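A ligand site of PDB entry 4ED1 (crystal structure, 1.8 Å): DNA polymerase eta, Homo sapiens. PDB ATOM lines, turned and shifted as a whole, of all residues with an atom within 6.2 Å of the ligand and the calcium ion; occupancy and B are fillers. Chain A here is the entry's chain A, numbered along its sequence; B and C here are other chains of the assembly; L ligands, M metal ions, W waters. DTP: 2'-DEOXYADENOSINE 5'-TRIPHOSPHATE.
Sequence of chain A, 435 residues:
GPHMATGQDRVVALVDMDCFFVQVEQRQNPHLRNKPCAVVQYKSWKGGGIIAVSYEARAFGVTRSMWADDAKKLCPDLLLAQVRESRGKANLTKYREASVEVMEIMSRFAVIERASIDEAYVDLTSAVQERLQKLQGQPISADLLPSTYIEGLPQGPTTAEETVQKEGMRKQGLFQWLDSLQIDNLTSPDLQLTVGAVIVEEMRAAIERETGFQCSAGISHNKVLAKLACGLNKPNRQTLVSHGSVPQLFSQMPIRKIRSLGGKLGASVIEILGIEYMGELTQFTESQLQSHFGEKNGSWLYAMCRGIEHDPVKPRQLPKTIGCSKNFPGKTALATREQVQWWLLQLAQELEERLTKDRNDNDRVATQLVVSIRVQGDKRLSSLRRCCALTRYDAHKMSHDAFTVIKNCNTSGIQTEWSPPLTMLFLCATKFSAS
A nitrogen (N6) of the ligand is in hydrogen-bond range of O4 of DT 4 of chain B (3.1 Å).
An oxygen (O2G) of the ligand is in hydrogen-bond range of the side-chain hydroxyl of Tyr 55 (2.6 Å).
An oxygen (O2B) of the ligand is in salt-bridge range of the guanidinium group of Arg 64 (3.1 Å).
O1G of the ligand is in salt-bridge range of NH1 of Arg 58 (3.2 Å).
O3' of the ligand lies within hydrogen-bond range of N of Phe 21 (3.2 Å).
An oxygen (O3') of the ligand lies within hydrogen-bond range of the backbone NH (N) of Phe 20, 3.5 Å away.
An oxygen (O2G) of the ligand sits at hydrogen-bond distance from the backbone NH (N) of Cys 19, 2.8 Å away.
The side-chain amino group of Lys 234 is in salt-bridge range of an oxygen (O2G) of the ligand (3.3 Å).
Water W1 lies within hydrogen-bond range of N7 of the ligand (2.8 Å) and NH1 of Arg 64 (3.4 Å).
Water W3 lies within hydrogen-bond range of OG of Ser 116 (2.5 Å), O3' of DT 8 of chain C (2.7 Å) and O4' of the ligand (2.9 Å).
Water W6 bridges NZ of Lys 227 and O1A of the ligand.
Water W2 lies within hydrogen-bond range of O2 of DT 8 of chain C and an oxygen (O4') of the ligand.
Within 4 Å of the calcium ion: Asp 16, Met 17 and Asp 118.
Along chain A the residues within 4 Å of the calcium ion span positions 16 to 118.
The nearest printed residue that does not touch the calcium ion is Lys 234 (4.1 Å).
A nitrogen (N1) of the ligand lies close to N1 of DA 5 of chain B (3.4 Å).
O3' of DT 8 of chain C lies close to an oxygen (O2A) of the ligand.
Residues that only touch the ligand: Ile 51, Asp 18, Ala 52, DT 3 of chain B and Ile 117.
Hydrophobic or aromatic side chains that line the ligand: Phe 20, Phe 21, Ile 51, Ala 52, Tyr 55 and Ile 117.
Of the 25 residues printed, 18 come within 4 Å of the ligand.
NZ of Lys 227 is in salt-bridge range of OP2 of DT 8 of chain C (3.4 Å).
NE of Arg 64 sits at hydrogen-bond distance from O of Ile 51 (2.8 Å).
OH of Tyr 55 lies close to NH1 of Arg 58, at 3.3 Å.
The backbone carbonyl oxygen (O) of Asp 16 sits at hydrogen-bond distance from the side-chain amino group (NZ) of Lys 234.
O2 of DT 4 of chain B lies within hydrogen-bond range of NE2 of Gln 41.
The guanidinium group of Arg 58 lies within hydrogen-bond range of the backbone carbonyl oxygen of Val 53, 2.9 Å away.
The side-chain hydroxyl of Ser 116 sits at hydrogen-bond distance from O3' of DT 8 of chain C.
The side-chain amino group (NZ) of Lys 234 lies within salt-bridge range of the side-chain carboxylate (OD1) of Asp 18 (2.7 Å).
The calcium ion is bound by O1B of the ligand (2.3 Å).
An oxygen (O3G) of the ligand is bound to the calcium ion, at 2.3 Å.
O of Met 17 binds the calcium ion (2.4 Å).
The calcium ion is bound by the side-chain carboxylate (OD1) of Asp 118, 2.4 Å away.
O2A of the ligand binds the calcium ion (2.4 Å).
The calcium ion is bound by OD2 of Asp 16 (2.6 Å).
The side-chain carboxylate (OD1) of Asp 16 binds the calcium ion (2.7 Å).
The calcium ion has seven donor atoms within binding distance.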
ATOM      1  N   ASP A  16       3.963   3.787  11.755  1.00  0.00           N
ATOM      2  CA  ASP A  16       3.422   2.441  11.833  1.00  0.00           C
ATOM      3  C   ASP A  16       4.524   1.396  11.769  1.00  0.00           C
ATOM      4  O   ASP A  16       5.327   1.394  10.851  1.00  0.00           O
ATOM      5  CB  ASP A  16       2.449   2.222  10.674  1.00  0.00           C
ATOM      6  CG  ASP A  16       2.014   0.792  10.561  1.00  0.00           C
ATOM      7  OD1 ASP A  16       2.418   0.141   9.578  1.00  0.00           O
ATOM      8  OD2 ASP A  16       1.295   0.314  11.450  1.00  0.00           O
ATOM      9  N   MET A  17       4.566   0.495  12.761  1.00  0.00           N
ATOM     10  CA  MET A  17       5.639  -0.515  12.817  1.00  0.00           C
ATOM     11  C   MET A  17       5.504  -1.530  11.682  1.00  0.00           C
ATOM     12  O   MET A  17       4.408  -1.935  11.325  1.00  0.00           O
ATOM     13  CB  MET A  17       5.587  -1.285  14.150  1.00  0.00           C
ATOM     14  CG  MET A  17       5.502  -0.404  15.399  1.00  0.00           C
ATOM     15  SD  MET A  17       6.815   0.820  15.447  1.00  0.00           S
ATOM     16  CE  MET A  17       8.248  -0.172  15.662  1.00  0.00           C
ATOM     17  N   ASP A  18       6.612  -1.935  11.091  1.00  0.00           N
ATOM     18  CA  ASP A  18       6.571  -2.928  10.021  1.00  0.00           C
ATOM     19  C   ASP A  18       6.292  -4.311  10.617  1.00  0.00           C
ATOM     20  O   ASP A  18       6.868  -4.682  11.646  1.00  0.00           O
ATOM     21  CB  ASP A  18       7.896  -2.941   9.258  1.00  0.00           C
ATOM     22  CG  ASP A  18       8.184  -1.604   8.571  1.00  0.00           C
ATOM     23  OD1 ASP A  18       7.235  -0.886   8.227  1.00  0.00           O
ATOM     24  OD2 ASP A  18       9.371  -1.300   8.347  1.00  0.00           O
ATOM     25  N   CYS A  19       5.396  -5.063   9.954  1.00  0.00           N
ATOM     26  CA  CYS A  19       4.993  -6.411  10.396  1.00  0.00           C
ATOM     27  C   CYS A  19       5.185  -6.620  11.895  1.00  0.00           C
ATOM     28  O   CYS A  19       6.019  -7.402  12.324  1.00  0.00           O
ATOM     29  CB  CYS A  19       5.707  -7.503   9.582  1.00  0.00           C
ATOM     30  SG  CYS A  19       7.509  -7.467   9.513  1.00  0.00           S
ATOM     31  N   PHE A  20       4.376  -5.929  12.687  1.00  0.00           N
ATOM     32  CA  PHE A  20       4.721  -5.701  14.089  1.00  0.00           C
ATOM     33  C   PHE A  20       4.885  -6.967  14.940  1.00  0.00           C
ATOM     34  O   PHE A  20       5.936  -7.145  15.564  1.00  0.00           O
ATOM     35  CB  PHE A  20       3.727  -4.735  14.751  1.00  0.00           C
ATOM     36  CG  PHE A  20       4.051  -4.417  16.174  1.00  0.00           C
ATOM     37  CD1 PHE A  20       5.308  -3.997  16.532  1.00  0.00           C
ATOM     38  CD2 PHE A  20       3.081  -4.526  17.156  1.00  0.00           C
ATOM     39  CE1 PHE A  20       5.617  -3.692  17.853  1.00  0.00           C
ATOM     40  CE2 PHE A  20       3.368  -4.219  18.487  1.00  0.00           C
ATOM     41  CZ  PHE A  20       4.633  -3.799  18.833  1.00  0.00           C
ATOM     42  N   PHE A  21       3.887  -7.852  14.983  1.00  0.00           N
ATOM     43  CA  PHE A  21       4.014  -9.016  15.871  1.00  0.00           C
ATOM     44  C   PHE A  21       5.187  -9.916  15.456  1.00  0.00           C
ATOM     45  O   PHE A  21       5.818 -10.545  16.301  1.00  0.00           O
ATOM     46  CB  PHE A  21       2.727  -9.874  15.936  1.00  0.00           C
ATOM     47  CG  PHE A  21       1.562  -9.215  16.628  1.00  0.00           C
ATOM     48  CD1 PHE A  21       1.566  -7.861  16.910  1.00  0.00           C
ATOM     49  CD2 PHE A  21       0.475  -9.981  17.010  1.00  0.00           C
ATOM     50  CE1 PHE A  21       0.487  -7.275  17.549  1.00  0.00           C
ATOM     51  CE2 PHE A  21      -0.612  -9.399  17.651  1.00  0.00           C
ATOM     52  CZ  PHE A  21      -0.605  -8.040  17.917  1.00  0.00           C
ATOM     53  N   VAL A  22       5.467  -9.975  14.152  1.00  0.00           N
ATOM     54  CA  VAL A  22       6.666 -10.667  13.680  1.00  0.00           C
ATOM     55  C   VAL A  22       7.980 -10.071  14.224  1.00  0.00           C
ATOM     56  O   VAL A  22       8.878 -10.815  14.693  1.00  0.00           O
ATOM     57  CB  VAL A  22       6.716 -10.723  12.138  1.00  0.00           C
ATOM     58  CG1 VAL A  22       8.095 -11.191  11.658  1.00  0.00           C
ATOM     59  CG2 VAL A  22       5.653 -11.662  11.617  1.00  0.00           C
ATOM     60  N   GLN A  41      -2.042 -17.969  15.614  1.00  0.00           N
ATOM     61  CA  GLN A  41      -2.703 -18.277  16.865  1.00  0.00           C
ATOM     62  C   GLN A  41      -3.454 -19.606  16.782  1.00  0.00           C
ATOM     63  O   GLN A  41      -4.078 -19.922  15.763  1.00  0.00           O
ATOM     64  CB  GLN A  41      -3.574 -17.130  17.386  1.00  0.00           C
ATOM     65  CG  GLN A  41      -4.712 -16.710  16.540  1.00  0.00           C
ATOM     66  CD  GLN A  41      -5.250 -15.337  16.941  1.00  0.00           C
ATOM     67  OE1 GLN A  41      -4.802 -14.733  17.919  1.00  0.00           O
ATOM     68  NE2 GLN A  41      -6.203 -14.836  16.174  1.00  0.00           N
ATOM     69  N   ILE A  51      -1.688 -14.197  11.796  1.00  0.00           N
ATOM     70  CA  ILE A  51      -2.073 -12.810  12.101  1.00  0.00           C
ATOM     71  C   ILE A  51      -1.041 -11.735  11.709  1.00  0.00           C
ATOM     72  O   ILE A  51      -1.387 -10.560  11.688  1.00  0.00           O
ATOM     73  CB  ILE A  51      -2.542 -12.629  13.563  1.00  0.00           C
ATOM     74  CG1 ILE A  51      -1.454 -13.041  14.558  1.00  0.00           C
ATOM     75  CG2 ILE A  51      -3.831 -13.427  13.830  1.00  0.00           C
ATOM     76  CD1 ILE A  51      -1.775 -12.584  15.974  1.00  0.00           C
ATOM     77  N   ALA A  52       0.182 -12.154  11.391  1.00  0.00           N
ATOM     78  CA  ALA A  52       1.260 -11.251  10.939  1.00  0.00           C
ATOM     79  C   ALA A  52       2.283 -11.995  10.076  1.00  0.00           C
ATOM     80  O   ALA A  52       2.573 -13.168  10.324  1.00  0.00           O
ATOM     81  CB  ALA A  52       1.964 -10.583  12.134  1.00  0.00           C
ATOM     82  N   VAL A  53       2.856 -11.305   9.090  1.00  0.00           N
ATOM     83  CA  VAL A  53       3.678 -11.951   8.060  1.00  0.00           C
ATOM     84  C   VAL A  53       4.915 -11.116   7.740  1.00  0.00           C
ATOM     85  O   VAL A  53       4.798  -9.927   7.457  1.00  0.00           O
ATOM     86  CB  VAL A  53       2.864 -12.110   6.761  1.00  0.00           C
ATOM     87  CG1 VAL A  53       3.643 -12.896   5.715  1.00  0.00           C
ATOM     88  CG2 VAL A  53       1.538 -12.782   7.036  1.00  0.00           C
ATOM     89  N   TYR A  55       8.033  -9.578   5.565  1.00  0.00           N
ATOM     90  CA  TYR A  55       8.142  -9.207   4.159  1.00  0.00           C
ATOM     91  C   TYR A  55       8.770 -10.306   3.295  1.00  0.00           C
ATOM     92  O   TYR A  55       8.384 -10.483   2.148  1.00  0.00           O
ATOM     93  CB  TYR A  55       8.839  -7.860   4.007  1.00  0.00           C
ATOM     94  CG  TYR A  55       7.891  -6.748   4.388  1.00  0.00           C
ATOM     95  CD1 TYR A  55       7.664  -6.451   5.726  1.00  0.00           C
ATOM     96  CD2 TYR A  55       7.171  -6.059   3.422  1.00  0.00           C
ATOM     97  CE1 TYR A  55       6.753  -5.470   6.092  1.00  0.00           C
ATOM     98  CE2 TYR A  55       6.276  -5.068   3.782  1.00  0.00           C
ATOM     99  CZ  TYR A  55       6.063  -4.779   5.114  1.00  0.00           C
ATOM    100  OH  TYR A  55       5.156  -3.793   5.464  1.00  0.00           O
ATOM    101  N   ARG A  58       5.883 -12.628   2.592  1.00  0.00           N
ATOM    102  CA  ARG A  58       4.909 -12.021   1.665  1.00  0.00           C
ATOM    103  C   ARG A  58       5.316 -12.248   0.194  1.00  0.00           C
ATOM    104  O   ARG A  58       4.446 -12.393  -0.680  1.00  0.00           O
ATOM    105  CB  ARG A  58       4.735 -10.531   1.949  1.00  0.00           C
ATOM    106  CG  ARG A  58       4.197 -10.235   3.339  1.00  0.00           C
ATOM    107  CD  ARG A  58       4.104  -8.748   3.606  1.00  0.00           C
ATOM    108  NE  ARG A  58       3.950  -8.503   5.034  1.00  0.00           N
ATOM    109  CZ  ARG A  58       3.529  -7.368   5.571  1.00  0.00           C
ATOM    110  NH1 ARG A  58       3.203  -6.340   4.788  1.00  0.00           N
ATOM    111  NH2 ARG A  58       3.427  -7.254   6.886  1.00  0.00           N
ATOM    112  N   ARG A  64      -2.101 -12.507   5.944  1.00  0.00           N
ATOM    113  CA  ARG A  64      -2.976 -12.608   7.110  1.00  0.00           C
ATOM    114  C   ARG A  64      -4.310 -13.329   6.784  1.00  0.00           C
ATOM    115  O   ARG A  64      -4.814 -13.249   5.670  1.00  0.00           O
ATOM    116  CB  ARG A  64      -3.206 -11.200   7.690  1.00  0.00           C
ATOM    117  CG  ARG A  64      -4.301 -11.063   8.737  1.00  0.00           C
ATOM    118  CD  ARG A  64      -4.344  -9.617   9.256  1.00  0.00           C
ATOM    119  NE  ARG A  64      -3.052  -9.240   9.816  1.00  0.00           N
ATOM    120  CZ  ARG A  64      -2.374  -8.137   9.502  1.00  0.00           C
ATOM    121  NH1 ARG A  64      -2.856  -7.269   8.624  1.00  0.00           N
ATOM    122  NH2 ARG A  64      -1.196  -7.910  10.074  1.00  0.00           N
ATOM    123  N   SER A 116      -3.730   2.374  17.030  1.00  0.00           N
ATOM    124  CA  SER A 116      -3.848   0.915  17.081  1.00  0.00           C
ATOM    125  C   SER A 116      -2.699   0.389  17.916  1.00  0.00           C
ATOM    126  O   SER A 116      -1.885   1.167  18.385  1.00  0.00           O
ATOM    127  CB  SER A 116      -3.788   0.326  15.666  1.00  0.00           C
ATOM    128  OG  SER A 116      -3.804  -1.091  15.696  1.00  0.00           O
ATOM    129  N   ILE A 117      -2.616  -0.932  18.081  1.00  0.00           N
ATOM    130  CA  ILE A 117      -1.516  -1.504  18.871  1.00  0.00           C
ATOM    131  C   ILE A 117      -0.139  -1.076  18.355  1.00  0.00           C
ATOM    132  O   ILE A 117       0.842  -1.004  19.105  1.00  0.00           O
ATOM    133  CB  ILE A 117      -1.589  -3.055  18.929  1.00  0.00           C
ATOM    134  CG1 ILE A 117      -0.677  -3.606  20.020  1.00  0.00           C
ATOM    135  CG2 ILE A 117      -1.261  -3.671  17.575  1.00  0.00           C
ATOM    136  CD1 ILE A 117      -1.042  -5.027  20.442  1.00  0.00           C
ATOM    137  N   ASP A 118      -0.042  -0.788  17.054  1.00  0.00           N
ATOM    138  CA  ASP A 118       1.280  -0.487  16.512  1.00  0.00           C
ATOM    139  C   ASP A 118       1.397   0.810  15.683  1.00  0.00           C
ATOM    140  O   ASP A 118       2.380   0.981  14.951  1.00  0.00           O
ATOM    141  CB  ASP A 118       1.790  -1.672  15.686  1.00  0.00           C
ATOM    142  CG  ASP A 118       1.266  -1.641  14.288  1.00  0.00           C
ATOM    143  OD1 ASP A 118       2.020  -2.068  13.406  1.00  0.00           O
ATOM    144  OD2 ASP A 118       0.127  -1.171  14.054  1.00  0.00           O
ATOM    145  N   GLU A 119       0.419   1.700  15.802  1.00  0.00           N
ATOM    146  CA  GLU A 119       0.563   2.968  15.105  1.00  0.00           C
ATOM    147  C   GLU A 119       0.064   4.163  15.911  1.00  0.00           C
ATOM    148  O   GLU A 119      -0.772   4.047  16.810  1.00  0.00           O
ATOM    149  CB  GLU A 119      -0.086   2.931  13.720  1.00  0.00           C
ATOM    150  CG  GLU A 119      -1.583   2.994  13.754  1.00  0.00           C
ATOM    151  CD  GLU A 119      -2.201   2.381  12.515  1.00  0.00           C
ATOM    152  OE1 GLU A 119      -2.451   1.165  12.535  1.00  0.00           O
ATOM    153  OE2 GLU A 119      -2.431   3.112  11.530  1.00  0.00           O
ATOM    154  N   LYS A 227      -1.642   8.781   6.735  1.00  0.00           N
ATOM    155  CA  LYS A 227      -1.867   7.336   6.744  1.00  0.00           C
ATOM    156  C   LYS A 227      -1.674   6.737   5.345  1.00  0.00           C
ATOM    157  O   LYS A 227      -0.984   5.731   5.177  1.00  0.00           O
ATOM    158  CB  LYS A 227      -3.282   7.011   7.260  1.00  0.00           C
ATOM    159  CG  LYS A 227      -3.684   5.520   7.168  1.00  0.00           C
ATOM    160  CD  LYS A 227      -2.835   4.649   8.086  1.00  0.00           C
ATOM    161  CE  LYS A 227      -3.286   3.196   8.061  1.00  0.00           C
ATOM    162  NZ  LYS A 227      -2.275   2.301   8.703  1.00  0.00           N
ATOM    163  N   LYS A 234       6.729   0.872   1.906  1.00  0.00           N
ATOM    164  CA  LYS A 234       6.989   0.034   3.077  1.00  0.00           C
ATOM    165  C   LYS A 234       7.822  -1.126   2.562  1.00  0.00           C
ATOM    166  O   LYS A 234       7.682  -1.500   1.398  1.00  0.00           O
ATOM    167  CB  LYS A 234       5.676  -0.507   3.652  1.00  0.00           C
ATOM    168  CG  LYS A 234       5.074   0.297   4.783  1.00  0.00           C
ATOM    169  CD  LYS A 234       4.058  -0.563   5.563  1.00  0.00           C
ATOM    170  CE  LYS A 234       3.711   0.037   6.938  1.00  0.00           C
ATOM    171  NZ  LYS A 234       4.510  -0.565   8.070  1.00  0.00           N
ATOM    172  N   PRO A 235       8.690  -1.706   3.403  1.00  0.00           N
ATOM    173  CA  PRO A 235       8.971  -1.407   4.811  1.00  0.00           C
ATOM    174  C   PRO A 235      10.153  -0.455   4.991  1.00  0.00           C
ATOM    175  O   PRO A 235      10.886  -0.175   4.044  1.00  0.00           O
ATOM    176  CB  PRO A 235       9.363  -2.779   5.362  1.00  0.00           C
ATOM    177  CG  PRO A 235      10.077  -3.427   4.192  1.00  0.00           C
ATOM    178  CD  PRO A 235       9.384  -2.921   2.953  1.00  0.00           C
ATOM    179  P    DT B   3     -13.421 -19.631   8.047  1.00  0.00           P
ATOM    180  OP1  DT B   3     -14.728 -19.947   7.443  1.00  0.00           O
ATOM    181  OP2  DT B   3     -12.177 -19.722   7.234  1.00  0.00           O
ATOM    182  O5'  DT B   3     -13.533 -18.162   8.654  1.00  0.00           O
ATOM    183  C5'  DT B   3     -12.376 -17.334   8.759  1.00  0.00           C
ATOM    184  C4'  DT B   3     -11.610 -17.622  10.024  1.00  0.00           C
ATOM    185  O4'  DT B   3     -10.332 -16.950   9.965  1.00  0.00           O
ATOM    186  C3'  DT B   3     -12.293 -17.161  11.313  1.00  0.00           C
ATOM    187  O3'  DT B   3     -12.176 -18.175  12.292  1.00  0.00           O
ATOM    188  C2'  DT B   3     -11.517 -15.895  11.709  1.00  0.00           C
ATOM    189  C1'  DT B   3     -10.135 -16.164  11.128  1.00  0.00           C
ATOM    190  N1   DT B   3      -9.394 -14.931  10.692  1.00  0.00           N
ATOM    191  C2   DT B   3      -8.165 -14.622  11.234  1.00  0.00           C
ATOM    192  O2   DT B   3      -7.605 -15.289  12.088  1.00  0.00           O
ATOM    193  N3   DT B   3      -7.591 -13.467  10.743  1.00  0.00           N
ATOM    194  C4   DT B   3      -8.121 -12.632   9.775  1.00  0.00           C
ATOM    195  O4   DT B   3      -7.523 -11.617   9.394  1.00  0.00           O
ATOM    196  C5   DT B   3      -9.411 -13.016   9.243  1.00  0.00           C
ATOM    197  C7   DT B   3     -10.092 -12.184   8.181  1.00  0.00           C
ATOM    198  C6   DT B   3      -9.977 -14.136   9.711  1.00  0.00           C
ATOM    199  P    DT B   4     -12.711 -17.905  13.785  1.00  0.00           P
ATOM    200  OP1  DT B   4     -12.772 -19.206  14.486  1.00  0.00           O
ATOM    201  OP2  DT B   4     -13.904 -17.043  13.689  1.00  0.00           O
ATOM    202  O5'  DT B   4     -11.547 -17.033  14.445  1.00  0.00           O
ATOM    203  C5'  DT B   4     -10.351 -17.660  14.889  1.00  0.00           C
ATOM    204  C4'  DT B   4      -9.655 -16.759  15.898  1.00  0.00           C
ATOM    205  O4'  DT B   4      -9.105 -15.609  15.226  1.00  0.00           O
ATOM    206  C3'  DT B   4     -10.556 -16.210  16.990  1.00  0.00           C
ATOM    207  O3'  DT B   4      -9.760 -16.266  18.145  1.00  0.00           O
ATOM    208  C2'  DT B   4     -10.855 -14.774  16.536  1.00  0.00           C
ATOM    209  C1'  DT B   4      -9.538 -14.411  15.840  1.00  0.00           C
ATOM    210  N1   DT B   4      -9.593 -13.378  14.756  1.00  0.00           N
ATOM    211  C2   DT B   4      -8.532 -12.510  14.619  1.00  0.00           C
ATOM    212  O2   DT B   4      -7.555 -12.507  15.344  1.00  0.00           O
ATOM    213  N3   DT B   4      -8.636 -11.624  13.597  1.00  0.00           N
ATOM    214  C4   DT B   4      -9.664 -11.500  12.696  1.00  0.00           C
ATOM    215  O4   DT B   4      -9.628 -10.646  11.814  1.00  0.00           O
ATOM    216  C5   DT B   4     -10.747 -12.437  12.866  1.00  0.00           C
ATOM    217  C7   DT B   4     -11.921 -12.376  11.925  1.00  0.00           C
ATOM    218  C6   DT B   4     -10.669 -13.325  13.876  1.00  0.00           C
ATOM    219  P    DA B   5     -10.297 -15.697  19.553  1.00  0.00           P
ATOM    220  OP1  DA B   5      -9.802 -16.588  20.607  1.00  0.00           O
ATOM    221  OP2  DA B   5     -11.756 -15.431  19.412  1.00  0.00           O
ATOM    222  O5'  DA B   5      -9.587 -14.265  19.659  1.00  0.00           O
ATOM    223  C5'  DA B   5      -8.186 -14.172  19.900  1.00  0.00           C
ATOM    224  C4'  DA B   5      -7.822 -12.721  20.163  1.00  0.00           C
ATOM    225  O4'  DA B   5      -7.937 -11.962  18.923  1.00  0.00           O
ATOM    226  C3'  DA B   5      -8.687 -12.000  21.199  1.00  0.00           C
ATOM    227  O3'  DA B   5      -7.820 -11.153  21.941  1.00  0.00           O
ATOM    228  C2'  DA B   5      -9.630 -11.189  20.328  1.00  0.00           C
ATOM    229  C1'  DA B   5      -8.701 -10.809  19.168  1.00  0.00           C
ATOM    230  N9   DA B   5      -9.396 -10.437  17.936  1.00  0.00           N
ATOM    231  C8   DA B   5     -10.550 -11.001  17.453  1.00  0.00           C
ATOM    232  N7   DA B   5     -10.956 -10.479  16.332  1.00  0.00           N
ATOM    233  C5   DA B   5     -10.010  -9.506  16.042  1.00  0.00           C
ATOM    234  C6   DA B   5      -9.886  -8.582  14.972  1.00  0.00           C
ATOM    235  N6   DA B   5     -10.753  -8.509  13.959  1.00  0.00           N
ATOM    236  N1   DA B   5      -8.832  -7.757  14.987  1.00  0.00           N
ATOM    237  C2   DA B   5      -7.966  -7.830  16.000  1.00  0.00           C
ATOM    238  N3   DA B   5      -7.974  -8.645  17.063  1.00  0.00           N
ATOM    239  C4   DA B   5      -9.039  -9.474  17.014  1.00  0.00           C
ATOM    240  P    DT C   8      -6.552   1.080   9.334  1.00  0.00           P
ATOM    241  OP1  DT C   8      -6.979   2.244  10.118  1.00  0.00           O
ATOM    242  OP2  DT C   8      -5.475   1.200   8.327  1.00  0.00           O
ATOM    243  O5'  DT C   8      -6.100  -0.089  10.309  1.00  0.00           O
ATOM    244  C5'  DT C   8      -5.424   0.274  11.493  1.00  0.00           C
ATOM    245  C4'  DT C   8      -5.013  -0.916  12.347  1.00  0.00           C
ATOM    246  O4'  DT C   8      -6.120  -1.751  12.761  1.00  0.00           O
ATOM    247  C3'  DT C   8      -3.932  -1.855  11.842  1.00  0.00           C
ATOM    248  O3'  DT C   8      -2.848  -1.794  12.765  1.00  0.00           O
ATOM    249  C2'  DT C   8      -4.578  -3.245  11.821  1.00  0.00           C
ATOM    250  C1'  DT C   8      -5.697  -3.104  12.839  1.00  0.00           C
ATOM    251  N1   DT C   8      -6.839  -4.011  12.533  1.00  0.00           N
ATOM    252  C2   DT C   8      -7.181  -4.958  13.458  1.00  0.00           C
ATOM    253  O2   DT C   8      -6.609  -5.080  14.520  1.00  0.00           O
ATOM    254  N3   DT C   8      -8.221  -5.771  13.119  1.00  0.00           N
ATOM    255  C4   DT C   8      -8.935  -5.724  11.940  1.00  0.00           C
ATOM    256  O4   DT C   8      -9.864  -6.494  11.713  1.00  0.00           O
ATOM    257  C5   DT C   8      -8.531  -4.713  10.988  1.00  0.00           C
ATOM    258  C7   DT C   8      -9.244  -4.575   9.685  1.00  0.00           C
ATOM    259  C6   DT C   8      -7.507  -3.915  11.324  1.00  0.00           C
HETATM  260  PG  DTP L   1       2.612  -3.859   7.951  1.00  0.00           P
HETATM  261  O1G DTP L   1       1.944  -4.063   6.607  1.00  0.00           O
HETATM  262  O2G DTP L   1       4.111  -3.839   7.823  1.00  0.00           O
HETATM  263  O3G DTP L   1       2.001  -2.732   8.735  1.00  0.00           O
HETATM  264  PB  DTP L   1       1.598  -5.326  10.223  1.00  0.00           P
HETATM  265  O1B DTP L   1       2.286  -4.388  11.169  1.00  0.00           O
HETATM  266  O2B DTP L   1       1.659  -6.784  10.615  1.00  0.00           O
HETATM  267  O3B DTP L   1       2.213  -5.216   8.740  1.00  0.00           O
HETATM  268  PA  DTP L   1      -0.941  -3.943  10.720  1.00  0.00           P
HETATM  269  O1A DTP L   1      -2.252  -3.964   9.948  1.00  0.00           O
HETATM  270  O2A DTP L   1      -0.325  -2.595  10.902  1.00  0.00           O
HETATM  271  O3A DTP L   1       0.049  -4.946   9.912  1.00  0.00           O
HETATM  272  O5' DTP L   1      -1.247  -4.594  12.160  1.00  0.00           O
HETATM  273  C5' DTP L   1      -0.360  -4.485  13.268  1.00  0.00           C
HETATM  274  C4' DTP L   1      -0.439  -5.758  14.107  1.00  0.00           C
HETATM  275  O4' DTP L   1      -1.752  -5.968  14.659  1.00  0.00           O
HETATM  276  C3' DTP L   1      -0.143  -6.993  13.277  1.00  0.00           C
HETATM  277  O3' DTP L   1       1.249  -7.318  13.296  1.00  0.00           O
HETATM  278  C2' DTP L   1      -0.957  -8.073  13.980  1.00  0.00           C
HETATM  279  C1' DTP L   1      -2.161  -7.330  14.526  1.00  0.00           C
HETATM  280  N9  DTP L   1      -3.313  -7.452  13.579  1.00  0.00           N
HETATM  281  C8  DTP L   1      -3.539  -6.713  12.479  1.00  0.00           C
HETATM  282  N7  DTP L   1      -4.698  -7.134  11.910  1.00  0.00           N
HETATM  283  C5  DTP L   1      -5.196  -8.130  12.686  1.00  0.00           C
HETATM  284  C6  DTP L   1      -6.326  -8.944  12.610  1.00  0.00           C
HETATM  285  N6  DTP L   1      -7.218  -8.787  11.598  1.00  0.00           N
HETATM  286  N1  DTP L   1      -6.536  -9.897  13.559  1.00  0.00           N
HETATM  287  C2  DTP L   1      -5.663 -10.046  14.564  1.00  0.00           C
HETATM  288  N3  DTP L   1      -4.556  -9.281  14.661  1.00  0.00           N
HETATM  289  C4  DTP L   1      -4.311  -8.322  13.722  1.00  0.00           C
HETATM  290 CA    CA M   1       2.058  -2.078  10.991  1.00  0.00          CA
HETATM  291  O   HOH W   1      -6.074  -6.666   9.503  1.00  0.00           O
HETATM  292  O   HOH W   2      -4.547  -5.469  16.128  1.00  0.00           O
HETATM  293  O   HOH W   3      -3.038  -3.383  14.924  1.00  0.00           O
HETATM  294  O   HOH W   4       0.935  -2.306   4.931  1.00  0.00           O
HETATM  295  O   HOH W   5       0.104  -1.039   7.723  1.00  0.00           O
HETATM  296  O   HOH W   6      -2.053  -0.762   9.280  1.00  0.00           O
HETATM  297  O   HOH W   7      -3.937  -9.616  17.361  1.00  0.00           O
HETATM  298  O   HOH W   8       1.604  -8.811   8.872  1.00  0.00           O
HETATM  299  O   HOH W   9      -0.216  -5.562   6.129  1.00  0.00           O
